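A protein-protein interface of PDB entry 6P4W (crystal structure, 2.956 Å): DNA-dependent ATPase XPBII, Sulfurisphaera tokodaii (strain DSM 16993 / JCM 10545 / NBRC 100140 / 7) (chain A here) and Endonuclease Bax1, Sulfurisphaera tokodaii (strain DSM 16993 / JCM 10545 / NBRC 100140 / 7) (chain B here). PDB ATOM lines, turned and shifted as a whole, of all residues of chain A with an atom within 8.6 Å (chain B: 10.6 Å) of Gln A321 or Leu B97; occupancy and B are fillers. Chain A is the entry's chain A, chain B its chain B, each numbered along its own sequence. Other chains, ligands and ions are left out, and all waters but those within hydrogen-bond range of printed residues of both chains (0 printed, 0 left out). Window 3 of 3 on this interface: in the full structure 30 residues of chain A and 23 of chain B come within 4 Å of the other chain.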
ATOM      1  N   ILE A 313      -9.898 -23.341  26.446  1.00  0.00           N
ATOM      2  CA  ILE A 313      -8.699 -22.874  25.761  1.00  0.00           C
ATOM      3  C   ILE A 313      -7.489 -23.020  26.665  1.00  0.00           C
ATOM      4  O   ILE A 313      -6.407 -23.444  26.235  1.00  0.00           O
ATOM      5  CB  ILE A 313      -8.904 -21.429  25.287  1.00  0.00           C
ATOM      6  CG1 ILE A 313      -9.941 -21.429  24.186  1.00  0.00           C
ATOM      7  CG2 ILE A 313      -7.644 -20.853  24.749  1.00  0.00           C
ATOM      8  CD1 ILE A 313     -10.485 -20.121  23.924  1.00  0.00           C
ATOM      9  N   GLU A 314      -7.666 -22.727  27.944  1.00  0.00           N
ATOM     10  CA  GLU A 314      -6.567 -22.903  28.870  1.00  0.00           C
ATOM     11  C   GLU A 314      -6.153 -24.367  28.945  1.00  0.00           C
ATOM     12  O   GLU A 314      -4.960 -24.690  28.877  1.00  0.00           O
ATOM     13  CB  GLU A 314      -6.980 -22.374  30.238  1.00  0.00           C
ATOM     14  CG  GLU A 314      -7.505 -20.969  30.197  1.00  0.00           C
ATOM     15  CD  GLU A 314      -6.527 -20.037  29.529  1.00  0.00           C
ATOM     16  OE1 GLU A 314      -5.305 -20.264  29.689  1.00  0.00           O
ATOM     17  OE2 GLU A 314      -6.975 -19.080  28.856  1.00  0.00           O
ATOM     18  N   LYS A 315      -7.137 -25.272  28.997  1.00  0.00           N
ATOM     19  CA  LYS A 315      -6.830 -26.694  28.969  1.00  0.00           C
ATOM     20  C   LYS A 315      -6.215 -27.085  27.642  1.00  0.00           C
ATOM     21  O   LYS A 315      -5.309 -27.930  27.596  1.00  0.00           O
ATOM     22  CB  LYS A 315      -8.087 -27.512  29.226  1.00  0.00           C
ATOM     23  CG  LYS A 315      -7.859 -29.010  29.105  1.00  0.00           C
ATOM     24  CD  LYS A 315      -6.767 -29.490  30.083  1.00  0.00           C
ATOM     25  CE  LYS A 315      -7.259 -29.556  31.530  1.00  0.00           C
ATOM     26  NZ  LYS A 315      -6.239 -30.112  32.476  1.00  0.00           N
ATOM     27  N   LEU A 316      -6.708 -26.492  26.549  1.00  0.00           N
ATOM     28  CA  LEU A 316      -6.162 -26.814  25.238  1.00  0.00           C
ATOM     29  C   LEU A 316      -4.681 -26.487  25.183  1.00  0.00           C
ATOM     30  O   LEU A 316      -3.884 -27.271  24.664  1.00  0.00           O
ATOM     31  CB  LEU A 316      -6.920 -26.062  24.147  1.00  0.00           C
ATOM     32  CG  LEU A 316      -6.411 -26.250  22.720  1.00  0.00           C
ATOM     33  CD1 LEU A 316      -6.369 -27.726  22.339  1.00  0.00           C
ATOM     34  CD2 LEU A 316      -7.284 -25.505  21.759  1.00  0.00           C
ATOM     35  N   ARG A 317      -4.285 -25.353  25.767  1.00  0.00           N
ATOM     36  CA  ARG A 317      -2.870 -25.019  25.805  1.00  0.00           C
ATOM     37  C   ARG A 317      -2.070 -26.109  26.495  1.00  0.00           C
ATOM     38  O   ARG A 317      -1.024 -26.516  25.998  1.00  0.00           O
ATOM     39  CB  ARG A 317      -2.660 -23.679  26.491  1.00  0.00           C
ATOM     40  CG  ARG A 317      -1.203 -23.282  26.531  1.00  0.00           C
ATOM     41  CD  ARG A 317      -1.034 -21.964  27.227  1.00  0.00           C
ATOM     42  NE  ARG A 317      -1.691 -20.894  26.492  1.00  0.00           N
ATOM     43  CZ  ARG A 317      -2.827 -20.332  26.884  1.00  0.00           C
ATOM     44  NH1 ARG A 317      -3.391 -19.360  26.162  1.00  0.00           N
ATOM     45  NH2 ARG A 317      -3.405 -20.761  28.006  1.00  0.00           N
ATOM     46  N   GLU A 318      -2.542 -26.594  27.644  1.00  0.00           N
ATOM     47  CA  GLU A 318      -1.857 -27.708  28.310  1.00  0.00           C
ATOM     48  C   GLU A 318      -1.708 -28.936  27.398  1.00  0.00           C
ATOM     49  O   GLU A 318      -0.663 -29.589  27.390  1.00  0.00           O
ATOM     50  CB  GLU A 318      -2.586 -28.094  29.599  1.00  0.00           C
ATOM     51  CG  GLU A 318      -2.901 -26.951  30.520  1.00  0.00           C
ATOM     52  CD  GLU A 318      -3.490 -27.416  31.848  1.00  0.00           C
ATOM     53  OE1 GLU A 318      -3.248 -28.584  32.229  1.00  0.00           O
ATOM     54  OE2 GLU A 318      -4.234 -26.626  32.487  1.00  0.00           O
ATOM     55  N   ILE A 319      -2.746 -29.284  26.649  1.00  0.00           N
ATOM     56  CA  ILE A 319      -2.676 -30.457  25.786  1.00  0.00           C
ATOM     57  C   ILE A 319      -1.677 -30.232  24.662  1.00  0.00           C
ATOM     58  O   ILE A 319      -0.875 -31.113  24.334  1.00  0.00           O
ATOM     59  CB  ILE A 319      -4.066 -30.788  25.219  1.00  0.00           C
ATOM     60  CG1 ILE A 319      -5.090 -30.960  26.324  1.00  0.00           C
ATOM     61  CG2 ILE A 319      -4.010 -32.039  24.406  1.00  0.00           C
ATOM     62  CD1 ILE A 319      -6.493 -30.859  25.791  1.00  0.00           C
ATOM     63  N   LEU A 320      -1.734 -29.069  24.021  1.00  0.00           N
ATOM     64  CA  LEU A 320      -0.807 -28.832  22.930  1.00  0.00           C
ATOM     65  C   LEU A 320       0.617 -28.813  23.430  1.00  0.00           C
ATOM     66  O   LEU A 320       1.526 -29.184  22.687  1.00  0.00           O
ATOM     67  CB  LEU A 320      -1.132 -27.521  22.224  1.00  0.00           C
ATOM     68  CG  LEU A 320      -2.484 -27.423  21.511  1.00  0.00           C
ATOM     69  CD1 LEU A 320      -2.651 -26.080  20.830  1.00  0.00           C
ATOM     70  CD2 LEU A 320      -2.643 -28.528  20.500  1.00  0.00           C
ATOM     71  N   GLN A 321       0.810 -28.483  24.699  1.00  0.00           N
ATOM     72  CA  GLN A 321       2.119 -28.561  25.318  1.00  0.00           C
ATOM     73  C   GLN A 321       2.526 -30.000  25.625  1.00  0.00           C
ATOM     74  O   GLN A 321       3.714 -30.328  25.585  1.00  0.00           O
ATOM     75  CB  GLN A 321       2.118 -27.712  26.591  1.00  0.00           C
ATOM     76  CG  GLN A 321       3.416 -27.743  27.363  1.00  0.00           C
ATOM     77  CD  GLN A 321       4.507 -26.913  26.723  1.00  0.00           C
ATOM     78  OE1 GLN A 321       4.429 -25.675  26.679  1.00  0.00           O
ATOM     79  NE2 GLN A 321       5.532 -27.592  26.206  1.00  0.00           N
ATOM     80  N   GLU A 322       1.575 -30.874  25.924  1.00  0.00           N
ATOM     81  CA  GLU A 322       1.909 -32.259  26.214  1.00  0.00           C
ATOM     82  C   GLU A 322       2.260 -33.032  24.953  1.00  0.00           C
ATOM     83  O   GLU A 322       3.039 -33.988  25.020  1.00  0.00           O
ATOM     84  CB  GLU A 322       0.730 -32.927  26.946  1.00  0.00           C
ATOM     85  CG  GLU A 322       1.029 -34.299  27.540  1.00  0.00           C
ATOM     86  CD  GLU A 322       2.077 -34.241  28.642  1.00  0.00           C
ATOM     87  OE1 GLU A 322       1.834 -33.579  29.682  1.00  0.00           O
ATOM     88  OE2 GLU A 322       3.165 -34.836  28.435  1.00  0.00           O
ATOM     89  N   TYR A 323       1.771 -32.592  23.800  1.00  0.00           N
ATOM     90  CA  TYR A 323       1.915 -33.337  22.555  1.00  0.00           C
ATOM     91  C   TYR A 323       2.583 -32.460  21.504  1.00  0.00           C
ATOM     92  O   TYR A 323       2.051 -32.270  20.408  1.00  0.00           O
ATOM     93  CB  TYR A 323       0.550 -33.855  22.092  1.00  0.00           C
ATOM     94  CG  TYR A 323      -0.114 -34.770  23.120  1.00  0.00           C
ATOM     95  CD1 TYR A 323       0.146 -36.133  23.142  1.00  0.00           C
ATOM     96  CD2 TYR A 323      -0.983 -34.259  24.086  1.00  0.00           C
ATOM     97  CE1 TYR A 323      -0.456 -36.971  24.084  1.00  0.00           C
ATOM     98  CE2 TYR A 323      -1.583 -35.086  25.029  1.00  0.00           C
ATOM     99  CZ  TYR A 323      -1.321 -36.446  25.025  1.00  0.00           C
ATOM    100  OH  TYR A 323      -1.918 -37.275  25.963  1.00  0.00           O
ATOM    101  N   LYS A 324       3.722 -31.870  21.879  1.00  0.00           N
ATOM    102  CA  LYS A 324       4.502 -31.042  20.969  1.00  0.00           C
ATOM    103  C   LYS A 324       4.816 -31.747  19.648  1.00  0.00           C
ATOM    104  O   LYS A 324       4.973 -31.084  18.619  1.00  0.00           O
ATOM    105  CB  LYS A 324       5.805 -30.604  21.650  1.00  0.00           C
ATOM    106  CG  LYS A 324       6.464 -31.659  22.543  1.00  0.00           C
ATOM    107  CD  LYS A 324       7.903 -31.273  22.900  1.00  0.00           C
ATOM    108  CE  LYS A 324       7.984 -30.666  24.289  1.00  0.00           C
ATOM    109  NZ  LYS A 324       9.221 -31.028  25.041  1.00  0.00           N
ATOM    110  N   ASN A 325       4.880 -33.077  19.642  1.00  0.00           N
ATOM    111  CA  ASN A 325       5.431 -33.800  18.503  1.00  0.00           C
ATOM    112  C   ASN A 325       4.393 -34.494  17.628  1.00  0.00           C
ATOM    113  O   ASN A 325       4.770 -35.052  16.589  1.00  0.00           O
ATOM    114  CB  ASN A 325       6.466 -34.826  18.988  1.00  0.00           C
ATOM    115  CG  ASN A 325       7.641 -34.170  19.722  1.00  0.00           C
ATOM    116  OD1 ASN A 325       8.161 -33.126  19.297  1.00  0.00           O
ATOM    117  ND2 ASN A 325       8.055 -34.777  20.833  1.00  0.00           N
ATOM    118  N   ILE A 328      -1.949 -32.578  15.239  1.00  0.00           N
ATOM    119  CA  ILE A 328      -3.189 -32.353  15.984  1.00  0.00           C
ATOM    120  C   ILE A 328      -4.166 -31.540  15.155  1.00  0.00           C
ATOM    121  O   ILE A 328      -3.782 -30.546  14.524  1.00  0.00           O
ATOM    122  CB  ILE A 328      -2.910 -31.665  17.330  1.00  0.00           C
ATOM    123  CG1 ILE A 328      -1.813 -32.431  18.062  1.00  0.00           C
ATOM    124  CG2 ILE A 328      -4.188 -31.577  18.179  1.00  0.00           C
ATOM    125  CD1 ILE A 328      -1.273 -31.733  19.252  1.00  0.00           C
ATOM    126  N   THR A 344      -5.513 -17.322  19.470  1.00  0.00           N
ATOM    127  CA  THR A 344      -4.811 -17.581  20.728  1.00  0.00           C
ATOM    128  C   THR A 344      -3.503 -18.324  20.527  1.00  0.00           C
ATOM    129  O   THR A 344      -2.556 -18.113  21.291  1.00  0.00           O
ATOM    130  CB  THR A 344      -5.694 -18.366  21.691  1.00  0.00           C
ATOM    131  OG1 THR A 344      -6.903 -17.643  21.919  1.00  0.00           O
ATOM    132  CG2 THR A 344      -4.998 -18.560  23.015  1.00  0.00           C
ATOM    133  N   PHE A 345      -3.429 -19.198  19.530  1.00  0.00           N
ATOM    134  CA  PHE A 345      -2.268 -20.057  19.340  1.00  0.00           C
ATOM    135  C   PHE A 345      -1.558 -19.838  18.010  1.00  0.00           C
ATOM    136  O   PHE A 345      -0.547 -20.502  17.749  1.00  0.00           O
ATOM    137  CB  PHE A 345      -2.682 -21.530  19.448  1.00  0.00           C
ATOM    138  CG  PHE A 345      -3.311 -21.890  20.757  1.00  0.00           C
ATOM    139  CD1 PHE A 345      -2.558 -21.920  21.910  1.00  0.00           C
ATOM    140  CD2 PHE A 345      -4.658 -22.209  20.839  1.00  0.00           C
ATOM    141  CE1 PHE A 345      -3.121 -22.257  23.119  1.00  0.00           C
ATOM    142  CE2 PHE A 345      -5.237 -22.543  22.052  1.00  0.00           C
ATOM    143  CZ  PHE A 345      -4.470 -22.570  23.191  1.00  0.00           C
ATOM    144  N   LEU A 346      -2.072 -18.950  17.162  1.00  0.00           N
ATOM    145  CA  LEU A 346      -1.538 -18.695  15.826  1.00  0.00           C
ATOM    146  C   LEU A 346      -1.441 -19.997  15.021  1.00  0.00           C
ATOM    147  O   LEU A 346      -0.372 -20.405  14.556  1.00  0.00           O
ATOM    148  CB  LEU A 346      -0.189 -17.973  15.909  1.00  0.00           C
ATOM    149  CG  LEU A 346      -0.156 -16.729  16.810  1.00  0.00           C
ATOM    150  CD1 LEU A 346       1.259 -16.232  17.043  1.00  0.00           C
ATOM    151  CD2 LEU A 346      -1.007 -15.616  16.237  1.00  0.00           C
ATOM    152  N   ILE A 347      -2.590 -20.651  14.859  1.00  0.00           N
ATOM    153  CA  ILE A 347      -2.668 -21.866  14.042  1.00  0.00           C
ATOM    154  C   ILE A 347      -3.721 -21.661  12.960  1.00  0.00           C
ATOM    155  O   ILE A 347      -4.621 -20.825  13.115  1.00  0.00           O
ATOM    156  CB  ILE A 347      -2.974 -23.109  14.893  1.00  0.00           C
ATOM    157  CG1 ILE A 347      -4.374 -23.014  15.486  1.00  0.00           C
ATOM    158  CG2 ILE A 347      -1.966 -23.248  16.025  1.00  0.00           C
ATOM    159  CD1 ILE A 347      -4.744 -24.191  16.321  1.00  0.00           C
ATOM    160  N   ARG A 372       1.846 -27.891  11.896  1.00  0.00           N
ATOM    161  CA  ARG A 372       1.746 -29.073  12.748  1.00  0.00           C
ATOM    162  C   ARG A 372       0.378 -29.198  13.417  1.00  0.00           C
ATOM    163  O   ARG A 372       0.000 -30.278  13.866  1.00  0.00           O
ATOM    164  CB  ARG A 372       2.896 -29.081  13.750  1.00  0.00           C
ATOM    165  CG  ARG A 372       2.801 -30.038  14.914  1.00  0.00           C
ATOM    166  CD  ARG A 372       3.823 -29.525  15.832  1.00  0.00           C
ATOM    167  NE  ARG A 372       3.443 -29.391  17.221  1.00  0.00           N
ATOM    168  CZ  ARG A 372       3.775 -28.303  17.913  1.00  0.00           C
ATOM    169  NH1 ARG A 372       3.438 -28.207  19.203  1.00  0.00           N
ATOM    170  NH2 ARG A 372       4.396 -27.284  17.290  1.00  0.00           N
ATOM    171  N   VAL A 373      -0.411 -28.134  13.437  1.00  0.00           N
ATOM    172  CA  VAL A 373      -1.704 -28.119  14.133  1.00  0.00           C
ATOM    173  C   VAL A 373      -2.640 -27.158  13.400  1.00  0.00           C
ATOM    174  O   VAL A 373      -2.219 -26.079  12.971  1.00  0.00           O
ATOM    175  CB  VAL A 373      -1.564 -27.701  15.629  1.00  0.00           C
ATOM    176  CG1 VAL A 373      -2.921 -27.435  16.280  1.00  0.00           C
ATOM    177  CG2 VAL A 373      -0.830 -28.750  16.412  1.00  0.00           C
ATOM    178  N   LEU A 391      -3.944 -36.971  16.719  1.00  0.00           N
ATOM    179  CA  LEU A 391      -4.614 -36.499  17.924  1.00  0.00           C
ATOM    180  C   LEU A 391      -5.743 -35.584  17.488  1.00  0.00           C
ATOM    181  O   LEU A 391      -5.503 -34.586  16.802  1.00  0.00           O
ATOM    182  CB  LEU A 391      -3.632 -35.762  18.838  1.00  0.00           C
ATOM    183  CG  LEU A 391      -4.212 -35.036  20.041  1.00  0.00           C
ATOM    184  CD1 LEU A 391      -4.845 -36.033  20.953  1.00  0.00           C
ATOM    185  CD2 LEU A 391      -3.139 -34.290  20.782  1.00  0.00           C
ATOM    186  N   ILE A 393      -8.785 -33.187  19.010  1.00  0.00           N
ATOM    187  CA  ILE A 393      -9.246 -32.516  20.212  1.00  0.00           C
ATOM    188  C   ILE A 393     -10.572 -31.877  19.878  1.00  0.00           C
ATOM    189  O   ILE A 393     -10.629 -30.913  19.102  1.00  0.00           O
ATOM    190  CB  ILE A 393      -8.252 -31.473  20.710  1.00  0.00           C
ATOM    191  CG1 ILE A 393      -6.866 -32.109  20.782  1.00  0.00           C
ATOM    192  CG2 ILE A 393      -8.726 -30.913  22.053  1.00  0.00           C
ATOM    193  CD1 ILE A 393      -5.930 -31.377  21.637  1.00  0.00           C
ATOM    194  N   TYR B  93       4.512 -19.776  12.351  1.00  0.00           N
ATOM    195  CA  TYR B  93       5.201 -19.856  13.631  1.00  0.00           C
ATOM    196  C   TYR B  93       4.598 -20.921  14.534  1.00  0.00           C
ATOM    197  O   TYR B  93       4.544 -20.743  15.759  1.00  0.00           O
ATOM    198  CB  TYR B  93       5.223 -18.473  14.293  1.00  0.00           C
ATOM    199  CG  TYR B  93       6.131 -17.501  13.538  1.00  0.00           C
ATOM    200  CD1 TYR B  93       7.439 -17.269  13.949  1.00  0.00           C
ATOM    201  CD2 TYR B  93       5.699 -16.874  12.377  1.00  0.00           C
ATOM    202  CE1 TYR B  93       8.274 -16.407  13.251  1.00  0.00           C
ATOM    203  CE2 TYR B  93       6.531 -16.018  11.674  1.00  0.00           C
ATOM    204  CZ  TYR B  93       7.815 -15.788  12.118  1.00  0.00           C
ATOM    205  OH  TYR B  93       8.645 -14.939  11.425  1.00  0.00           O
ATOM    206  N   GLY B  94       4.108 -22.010  13.931  1.00  0.00           N
ATOM    207  CA  GLY B  94       3.501 -23.120  14.626  1.00  0.00           C
ATOM    208  C   GLY B  94       2.469 -22.651  15.617  1.00  0.00           C
ATOM    209  O   GLY B  94       1.985 -21.517  15.542  1.00  0.00           O
ATOM    210  N   PRO B  95       2.108 -23.512  16.572  1.00  0.00           N
ATOM    211  CA  PRO B  95       1.305 -23.059  17.721  1.00  0.00           C
ATOM    212  C   PRO B  95       2.180 -22.450  18.806  1.00  0.00           C
ATOM    213  O   PRO B  95       3.144 -23.060  19.272  1.00  0.00           O
ATOM    214  CB  PRO B  95       0.609 -24.334  18.199  1.00  0.00           C
ATOM    215  CG  PRO B  95       1.465 -25.433  17.699  1.00  0.00           C
ATOM    216  CD  PRO B  95       2.070 -24.976  16.411  1.00  0.00           C
ATOM    217  N   VAL B  96       1.844 -21.232  19.192  1.00  0.00           N
ATOM    218  CA  VAL B  96       2.573 -20.505  20.213  1.00  0.00           C
ATOM    219  C   VAL B  96       1.847 -20.723  21.526  1.00  0.00           C
ATOM    220  O   VAL B  96       0.658 -20.407  21.646  1.00  0.00           O
ATOM    221  CB  VAL B  96       2.651 -19.010  19.878  1.00  0.00           C
ATOM    222  CG1 VAL B  96       3.323 -18.298  20.998  1.00  0.00           C
ATOM    223  CG2 VAL B  96       3.384 -18.776  18.561  1.00  0.00           C
ATOM    224  N   LEU B  97       2.545 -21.264  22.514  1.00  0.00           N
ATOM    225  CA  LEU B  97       1.902 -21.571  23.776  1.00  0.00           C
ATOM    226  C   LEU B  97       2.321 -20.642  24.899  1.00  0.00           C
ATOM    227  O   LEU B  97       1.673 -20.640  25.947  1.00  0.00           O
ATOM    228  CB  LEU B  97       2.185 -23.023  24.174  1.00  0.00           C
ATOM    229  CG  LEU B  97       1.935 -23.984  23.014  1.00  0.00           C
ATOM    230  CD1 LEU B  97       2.635 -25.296  23.238  1.00  0.00           C
ATOM    231  CD2 LEU B  97       0.449 -24.190  22.820  1.00  0.00           C
ATOM    232  N   ASP B  98       3.354 -19.825  24.698  1.00  0.00           N
ATOM    233  CA  ASP B  98       3.785 -18.821  25.664  1.00  0.00           C
ATOM    234  C   ASP B  98       3.183 -17.468  25.290  1.00  0.00           C
ATOM    235  O   ASP B  98       3.233 -17.065  24.124  1.00  0.00           O
ATOM    236  CB  ASP B  98       5.313 -18.742  25.709  1.00  0.00           C
ATOM    237  CG  ASP B  98       5.830 -17.822  26.806  1.00  0.00           C
ATOM    238  OD1 ASP B  98       7.068 -17.719  26.941  1.00  0.00           O
ATOM    239  OD2 ASP B  98       5.020 -17.212  27.536  1.00  0.00           O
ATOM    240  N   GLU B  99       2.598 -16.780  26.276  1.00  0.00           N
ATOM    241  CA  GLU B  99       1.964 -15.490  26.006  1.00  0.00           C
ATOM    242  C   GLU B  99       2.979 -14.439  25.557  1.00  0.00           C
ATOM    243  O   GLU B  99       2.693 -13.640  24.658  1.00  0.00           O
ATOM    244  CB  GLU B  99       1.215 -15.012  27.253  1.00  0.00           C
ATOM    245  CG  GLU B  99       0.284 -13.825  27.038  1.00  0.00           C
ATOM    246  CD  GLU B  99      -0.192 -13.208  28.351  1.00  0.00           C
ATOM    247  OE1 GLU B  99       0.351 -13.561  29.423  1.00  0.00           O
ATOM    248  OE2 GLU B  99      -1.113 -12.366  28.310  1.00  0.00           O
ATOM    249  N   LYS B 100       4.165 -14.415  26.174  1.00  0.00           N
ATOM    250  CA  LYS B 100       5.172 -13.434  25.776  1.00  0.00           C
ATOM    251  C   LYS B 100       5.710 -13.721  24.384  1.00  0.00           C
ATOM    252  O   LYS B 100       5.846 -12.803  23.566  1.00  0.00           O
ATOM    253  CB  LYS B 100       6.323 -13.399  26.777  1.00  0.00           C
ATOM    254  N   GLU B 101       6.009 -14.992  24.084  1.00  0.00           N
ATOM    255  CA  GLU B 101       6.502 -15.309  22.750  1.00  0.00           C
ATOM    256  C   GLU B 101       5.470 -14.959  21.691  1.00  0.00           C
ATOM    257  O   GLU B 101       5.831 -14.573  20.574  1.00  0.00           O
ATOM    258  CB  GLU B 101       6.876 -16.787  22.637  1.00  0.00           C
ATOM    259  CG  GLU B 101       7.565 -17.106  21.307  1.00  0.00           C
ATOM    260  CD  GLU B 101       7.907 -18.577  21.124  1.00  0.00           C
ATOM    261  OE1 GLU B 101       7.522 -19.410  21.982  1.00  0.00           O
ATOM    262  OE2 GLU B 101       8.569 -18.890  20.107  1.00  0.00           O
ATOM    263  N   ARG B 102       4.182 -15.028  22.038  1.00  0.00           N
ATOM    264  CA  ARG B 102       3.141 -14.674  21.081  1.00  0.00           C
ATOM    265  C   ARG B 102       3.240 -13.206  20.697  1.00  0.00           C
ATOM    266  O   ARG B 102       3.342 -12.868  19.512  1.00  0.00           O
ATOM    267  CB  ARG B 102       1.763 -14.988  21.661  1.00  0.00           C
ATOM    268  CG  ARG B 102       0.604 -14.626  20.746  1.00  0.00           C
ATOM    269  CD  ARG B 102      -0.742 -15.054  21.326  1.00  0.00           C
ATOM    270  NE  ARG B 102      -1.840 -14.645  20.457  1.00  0.00           N
ATOM    271  CZ  ARG B 102      -2.490 -13.491  20.565  1.00  0.00           C
ATOM    272  NH1 ARG B 102      -2.164 -12.635  21.522  1.00  0.00           N
ATOM    273  NH2 ARG B 102      -3.463 -13.188  19.718  1.00  0.00           N
ATOM    274  N   GLU B 103       3.230 -12.318  21.698  1.00  0.00           N
ATOM    275  CA  GLU B 103       3.308 -10.883  21.432  1.00  0.00           C
ATOM    276  C   GLU B 103       4.494 -10.549  20.549  1.00  0.00           C
ATOM    277  O   GLU B 103       4.380  -9.721  19.639  1.00  0.00           O
ATOM    278  CB  GLU B 103       3.386 -10.103  22.740  1.00  0.00           C
ATOM    279  CG  GLU B 103       2.176 -10.327  23.625  1.00  0.00           C
ATOM    280  CD  GLU B 103       2.259  -9.585  24.937  1.00  0.00           C
ATOM    281  OE1 GLU B 103       3.332  -9.013  25.232  1.00  0.00           O
ATOM    282  OE2 GLU B 103       1.251  -9.596  25.680  1.00  0.00           O
ATOM    283  N   ILE B 105       6.082 -12.644  18.360  1.00  0.00           N
ATOM    284  CA  ILE B 105       5.774 -13.108  17.006  1.00  0.00           C
ATOM    285  C   ILE B 105       4.898 -12.091  16.298  1.00  0.00           C
ATOM    286  O   ILE B 105       5.118 -11.766  15.127  1.00  0.00           O
ATOM    287  CB  ILE B 105       5.100 -14.492  17.031  1.00  0.00           C
ATOM    288  CG1 ILE B 105       5.992 -15.531  17.684  1.00  0.00           C
ATOM    289  CG2 ILE B 105       4.791 -14.954  15.627  1.00  0.00           C
ATOM    290  CD1 ILE B 105       7.273 -15.739  16.947  1.00  0.00           C
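Of chain B, only Leu B97 comes within 4 Å of Gln A321. Of the printed residues of chain A, Leu B97 touches Arg A317 (3.3 Å), Leu A320 (3.7 Å), Gln A321 (3.9 Å) and Phe A345 (3.9 Å). Of the printed residues of chain B, Leu A346 touches Gly B94 and Val B96. Of the printed residues of chain B, Phe A345 touches Gly B94, Pro B95, Val B96 and Leu B97. Glu B103 touches none of the printed residues of chain A. Asn A325 touches none of the printed residues of chain B. The nearest residue of chain B that does not touch Gln A321 is Asp B98 (6.3 Å). The nearest residue of chain A that does not touch Leu B97 is Arg A372 (5.0 Å).
The guanidinium group (NE) of Arg A372 sits at hydrogen-bond distance from the backbone carbonyl oxygen (O) of Lys A324 (2.7 Å). The backbone NH (N) of Ile A328 sits at hydrogen-bond distance from the backbone carbonyl oxygen (O) of Arg A372 (3.3 Å). The side-chain carboxylate (OE1) of Glu A314 is in salt-bridge range of the guanidinium group (NH2) of Arg A317 (2.6 Å).
Among the printed residues, pairs that only touch across the chains: Phe A345 with Pro B95 (3.2 Å), Arg A372 with Pro B95 (3.4 Å), Phe A345 with Gly B94 (3.5 Å), Ile A347 with Pro B95 (3.5 Å), Thr A344 with Arg B102 (3.6 Å), Leu A346 with Val B96 (3.6 Å), Leu A320 with Leu B97 (3.7 Å), Phe A345 with Leu B97 (3.9 Å), Gln A321 with Leu B97 (3.9 Å) and Thr A344 with Val B96 (3.96 Å).
The backbone carbonyl oxygen (O) of Leu A346 lies close to the backbone carbonyl oxygen (O) of Gly B94, 2.8 Å away. The guanidinium group (NE) of Arg A317 sits close to the backbone carbonyl oxygen (O) of Leu B97 (3.4 Å). The backbone NH (N) of Val B96 is in hydrogen-bond range of the backbone carbonyl oxygen (O) of Phe A345 (2.9 Å).
Hydrophobic or aromatic side chains of chain B within 4 Å of the printed part of chain A: Pro B95, Val B96 and Leu B97. Among the printed residues, no Asp or Glu carboxylate lies within 4 Å of a Lys or Arg side-chain nitrogen of the other chain.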
